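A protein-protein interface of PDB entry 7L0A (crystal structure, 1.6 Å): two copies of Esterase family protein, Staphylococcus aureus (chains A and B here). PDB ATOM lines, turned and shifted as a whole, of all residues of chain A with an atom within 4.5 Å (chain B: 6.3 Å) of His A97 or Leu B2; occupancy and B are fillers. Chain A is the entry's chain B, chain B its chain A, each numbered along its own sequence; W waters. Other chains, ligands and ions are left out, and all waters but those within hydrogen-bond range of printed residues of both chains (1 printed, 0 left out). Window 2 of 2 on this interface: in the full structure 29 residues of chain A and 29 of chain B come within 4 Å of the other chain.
Of the printed residues of chain B, His A97 touches Leu B2 (3.5 Å).
Of the printed residues of chain A, Leu B2 touches Pro A19, Thr A20, Gly A96 and His A97.
Of the printed residues of chain A, Val B3 touches Pro A19 (3.5 Å).
Printed residues of chain A within 4 Å of Phe B38: Pro A19 (3.7 Å).
Printed residues of chain B within 4 Å of Gly A96: Leu B2.
Ala A94 touches none of the printed residues of chain B.
The nearest printed residue of chain A that does not touch Leu B2 is Ile A21 (5.9 Å).
The nearest printed residue of chain A that does not touch Phe B38 is Thr A20 (6.6 Å).
Of the 6 printed residues of chain B, 4 touch a printed residue of chain A.
Hydrophobic or aromatic side chains of chain B that line the printed part of chain A: Leu B2, Pro B4 and Phe B38.
Hydrophobic or aromatic side chains of chain A within 4 Å of the printed part of chain B: Pro A19 and His A97.
Among the printed residues, no Asp or Glu carboxylate lies within 4 Å of a Lys or Arg side-chain nitrogen of the other chain.
Water W1 bridges the side-chain hydroxyl of Thr A20 (2.8 Å) and the backbone NH of Leu B2 (3.0 Å).
Among the printed residues, merely in contact across the chains: Pro A19 with Pro B4, His A97 with Leu B2, Pro A19 with Val B3, Thr A20 with Leu B2, Gly A96 with Leu B2, Pro A19 with Phe B38 and Pro A19 with Leu B2.
The backbone carbonyl oxygen (O) of Thr A20 sits at hydrogen-bond distance from a ring nitrogen (ND1) of His A97 (2.9 Å).
The side-chain carboxylate (OD2) of Asp A101 sits close to the backbone NH (N) of Gly A96 (3.4 Å).
The backbone NH (N) of His A97 is in hydrogen-bond range of the side-chain carboxylate (OD2) of Asp A101 (3.4 Å).
No position is printed for both chains.
Of the 7 pairs that touch across the chains among the printed residues, none has its exchanged pair printed and touching as well.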
ATOM      1  N   PRO A  19      -3.138   4.886  13.631  1.00  0.00           N
ATOM      2  CA  PRO A  19      -3.731   3.612  13.161  1.00  0.00           C
ATOM      3  C   PRO A  19      -4.891   3.153  14.014  1.00  0.00           C
ATOM      4  O   PRO A  19      -5.860   2.577  13.487  1.00  0.00           O
ATOM      5  CB  PRO A  19      -2.558   2.633  13.239  1.00  0.00           C
ATOM      6  CG  PRO A  19      -1.318   3.456  13.349  1.00  0.00           C
ATOM      7  CD  PRO A  19      -1.699   4.795  13.952  1.00  0.00           C
ATOM      8  N   THR A  20      -4.844   3.430  15.321  1.00  0.00           N
ATOM      9  CA  THR A  20      -5.879   2.938  16.223  1.00  0.00           C
ATOM     10  C   THR A  20      -7.182   3.687  16.035  1.00  0.00           C
ATOM     11  O   THR A  20      -8.237   3.069  15.886  1.00  0.00           O
ATOM     12  CB  THR A  20      -5.391   3.054  17.657  1.00  0.00           C
ATOM     13  OG1 THR A  20      -4.217   2.264  17.821  1.00  0.00           O
ATOM     14  CG2 THR A  20      -6.469   2.586  18.629  1.00  0.00           C
ATOM     15  N   ILE A  21      -7.126   5.023  16.017  1.00  0.00           N
ATOM     16  CA  ILE A  21      -8.331   5.830  15.849  1.00  0.00           C
ATOM     17  C   ILE A  21      -8.736   5.886  14.395  1.00  0.00           C
ATOM     18  O   ILE A  21      -9.925   5.983  14.085  1.00  0.00           O
ATOM     19  CB  ILE A  21      -8.093   7.245  16.429  1.00  0.00           C
ATOM     20  CG1 ILE A  21      -7.789   7.131  17.930  1.00  0.00           C
ATOM     21  CG2 ILE A  21      -9.326   8.142  16.184  1.00  0.00           C
ATOM     22  CD1 ILE A  21      -8.946   6.626  18.782  1.00  0.00           C
ATOM     23  N   MET A  93     -16.168   3.938  19.732  1.00  0.00           N
ATOM     24  CA  MET A  93     -15.313   3.127  18.881  1.00  0.00           C
ATOM     25  C   MET A  93     -15.440   1.645  19.217  1.00  0.00           C
ATOM     26  O   MET A  93     -15.821   1.253  20.327  1.00  0.00           O
ATOM     27  CB  MET A  93     -13.851   3.562  19.015  1.00  0.00           C
ATOM     28  CG  MET A  93     -13.654   5.041  18.822  1.00  0.00           C
ATOM     29  SD  MET A  93     -14.005   5.594  17.134  1.00  0.00           S
ATOM     30  CE  MET A  93     -12.586   4.953  16.244  1.00  0.00           C
ATOM     31  N   ALA A  94     -15.110   0.824  18.221  1.00  0.00           N
ATOM     32  CA  ALA A  94     -15.066  -0.615  18.407  1.00  0.00           C
ATOM     33  C   ALA A  94     -13.938  -1.030  19.356  1.00  0.00           C
ATOM     34  O   ALA A  94     -12.946  -0.319  19.558  1.00  0.00           O
ATOM     35  CB  ALA A  94     -14.897  -1.303  17.052  1.00  0.00           C
ATOM     36  N   TYR A  95     -14.105  -2.213  19.947  1.00  0.00           N
ATOM     37  CA  TYR A  95     -13.054  -2.806  20.761  1.00  0.00           C
ATOM     38  C   TYR A  95     -11.774  -2.879  19.937  1.00  0.00           C
ATOM     39  O   TYR A  95     -11.800  -3.269  18.757  1.00  0.00           O
ATOM     40  CB  TYR A  95     -13.501  -4.188  21.241  1.00  0.00           C
ATOM     41  CG  TYR A  95     -12.518  -4.903  22.147  1.00  0.00           C
ATOM     42  CD1 TYR A  95     -12.271  -4.454  23.441  1.00  0.00           C
ATOM     43  CD2 TYR A  95     -11.853  -6.042  21.712  1.00  0.00           C
ATOM     44  CE1 TYR A  95     -11.375  -5.116  24.272  1.00  0.00           C
ATOM     45  CE2 TYR A  95     -10.959  -6.709  22.533  1.00  0.00           C
ATOM     46  CZ  TYR A  95     -10.723  -6.241  23.812  1.00  0.00           C
ATOM     47  OH  TYR A  95      -9.834  -6.900  24.631  1.00  0.00           O
ATOM     48  N   GLY A  96     -10.659  -2.475  20.549  1.00  0.00           N
ATOM     49  CA  GLY A  96      -9.394  -2.406  19.868  1.00  0.00           C
ATOM     50  C   GLY A  96      -9.082  -1.062  19.259  1.00  0.00           C
ATOM     51  O   GLY A  96      -7.937  -0.818  18.879  1.00  0.00           O
ATOM     52  N   HIS A  97     -10.085  -0.188  19.138  1.00  0.00           N
ATOM     53  CA  HIS A  97      -9.904   1.114  18.510  1.00  0.00           C
ATOM     54  C   HIS A  97     -10.370   2.232  19.418  1.00  0.00           C
ATOM     55  O   HIS A  97     -10.720   3.314  18.927  1.00  0.00           O
ATOM     56  CB  HIS A  97     -10.660   1.158  17.192  1.00  0.00           C
ATOM     57  CG  HIS A  97     -10.203   0.116  16.229  1.00  0.00           C
ATOM     58  ND1 HIS A  97      -9.226   0.356  15.292  1.00  0.00           N
ATOM     59  CD2 HIS A  97     -10.545  -1.187  16.095  1.00  0.00           C
ATOM     60  CE1 HIS A  97      -9.010  -0.743  14.591  1.00  0.00           C
ATOM     61  NE2 HIS A  97      -9.790  -1.698  15.067  1.00  0.00           N
ATOM     62  N   SER A  98     -10.390   1.993  20.717  1.00  0.00           N
ATOM     63  CA  SER A  98     -10.976   2.898  21.694  1.00  0.00           C
ATOM     64  C   SER A  98      -9.878   3.608  22.481  1.00  0.00           C
ATOM     65  O   SER A  98      -8.685   3.359  22.283  1.00  0.00           O
ATOM     66  CB  SER A  98     -11.910   2.124  22.627  1.00  0.00           C
ATOM     67  OG  SER A  98     -13.053   1.604  21.934  1.00  0.00           O
ATOM     68  N   ASP A 101      -6.908   1.625  23.827  1.00  0.00           N
ATOM     69  CA  ASP A 101      -5.938   1.209  22.827  1.00  0.00           C
ATOM     70  C   ASP A 101      -5.144   2.404  22.324  1.00  0.00           C
ATOM     71  O   ASP A 101      -3.947   2.285  22.024  1.00  0.00           O
ATOM     72  CB  ASP A 101      -6.662   0.526  21.687  1.00  0.00           C
ATOM     73  CG  ASP A 101      -7.665  -0.513  22.203  1.00  0.00           C
ATOM     74  OD1 ASP A 101      -7.192  -1.618  22.573  1.00  0.00           O
ATOM     75  OD2 ASP A 101      -8.888  -0.208  22.295  1.00  0.00           O
ATOM     76  N   GLY B   1      -0.677  -4.203  19.018  1.00  0.00           N
ATOM     77  CA  GLY B   1      -0.781  -2.779  18.723  1.00  0.00           C
ATOM     78  C   GLY B   1      -0.866  -2.514  17.231  1.00  0.00           C
ATOM     79  O   GLY B   1      -0.076  -3.063  16.458  1.00  0.00           O
ATOM     80  N   LEU B   2      -1.810  -1.660  16.831  1.00  0.00           N
ATOM     81  CA  LEU B   2      -2.034  -1.408  15.415  1.00  0.00           C
ATOM     82  C   LEU B   2      -0.915  -0.552  14.822  1.00  0.00           C
ATOM     83  O   LEU B   2      -0.326   0.293  15.502  1.00  0.00           O
ATOM     84  CB  LEU B   2      -3.375  -0.711  15.220  1.00  0.00           C
ATOM     85  CG  LEU B   2      -4.542  -1.602  15.632  1.00  0.00           C
ATOM     86  CD1 LEU B   2      -5.790  -0.729  15.849  1.00  0.00           C
ATOM     87  CD2 LEU B   2      -4.798  -2.689  14.612  1.00  0.00           C
ATOM     88  N   VAL B   3      -0.652  -0.771  13.541  1.00  0.00           N
ATOM     89  CA  VAL B   3       0.402  -0.048  12.826  1.00  0.00           C
ATOM     90  C   VAL B   3      -0.187   0.584  11.575  1.00  0.00           C
ATOM     91  O   VAL B   3      -1.219   0.140  11.061  1.00  0.00           O
ATOM     92  CB  VAL B   3       1.585  -0.976  12.457  1.00  0.00           C
ATOM     93  CG1 VAL B   3       2.151  -1.630  13.691  1.00  0.00           C
ATOM     94  CG2 VAL B   3       1.225  -1.965  11.380  1.00  0.00           C
ATOM     95  N   PRO B   4       0.466   1.616  11.037  1.00  0.00           N
ATOM     96  CA  PRO B   4      -0.108   2.296   9.870  1.00  0.00           C
ATOM     97  C   PRO B   4      -0.223   1.401   8.650  1.00  0.00           C
ATOM     98  O   PRO B   4       0.663   0.595   8.349  1.00  0.00           O
ATOM     99  CB  PRO B   4       0.865   3.460   9.615  1.00  0.00           C
ATOM    100  CG  PRO B   4       1.603   3.647  10.888  1.00  0.00           C
ATOM    101  CD  PRO B   4       1.679   2.285  11.538  1.00  0.00           C
ATOM    102  N   PHE B  38       5.469   1.906  15.685  1.00  0.00           N
ATOM    103  CA  PHE B  38       4.239   1.616  16.402  1.00  0.00           C
ATOM    104  C   PHE B  38       4.248   0.240  17.044  1.00  0.00           C
ATOM    105  O   PHE B  38       3.293  -0.111  17.735  1.00  0.00           O
ATOM    106  CB  PHE B  38       3.064   1.736  15.425  1.00  0.00           C
ATOM    107  CG  PHE B  38       2.774   3.137  15.060  1.00  0.00           C
ATOM    108  CD1 PHE B  38       3.484   3.774  14.049  1.00  0.00           C
ATOM    109  CD2 PHE B  38       1.895   3.867  15.813  1.00  0.00           C
ATOM    110  CE1 PHE B  38       3.250   5.088  13.771  1.00  0.00           C
ATOM    111  CE2 PHE B  38       1.670   5.180  15.553  1.00  0.00           C
ATOM    112  CZ  PHE B  38       2.343   5.793  14.528  1.00  0.00           C
ATOM    113  N   ASN B  39       5.320  -0.520  16.864  1.00  0.00           N
ATOM    114  CA  ASN B  39       5.429  -1.905  17.316  1.00  0.00           C
ATOM    115  C   ASN B  39       6.501  -1.899  18.399  1.00  0.00           C
ATOM    116  O   ASN B  39       7.686  -1.736  18.106  1.00  0.00           O
ATOM    117  CB  ASN B  39       5.793  -2.814  16.147  1.00  0.00           C
ATOM    118  CG  ASN B  39       5.796  -4.268  16.540  1.00  0.00           C
ATOM    119  OD1 ASN B  39       5.942  -4.600  17.721  1.00  0.00           O
ATOM    120  ND2 ASN B  39       5.599  -5.144  15.559  1.00  0.00           N
HETATM  121  O   HOH W   1      -3.679  -0.350  18.818  1.00  0.00           O
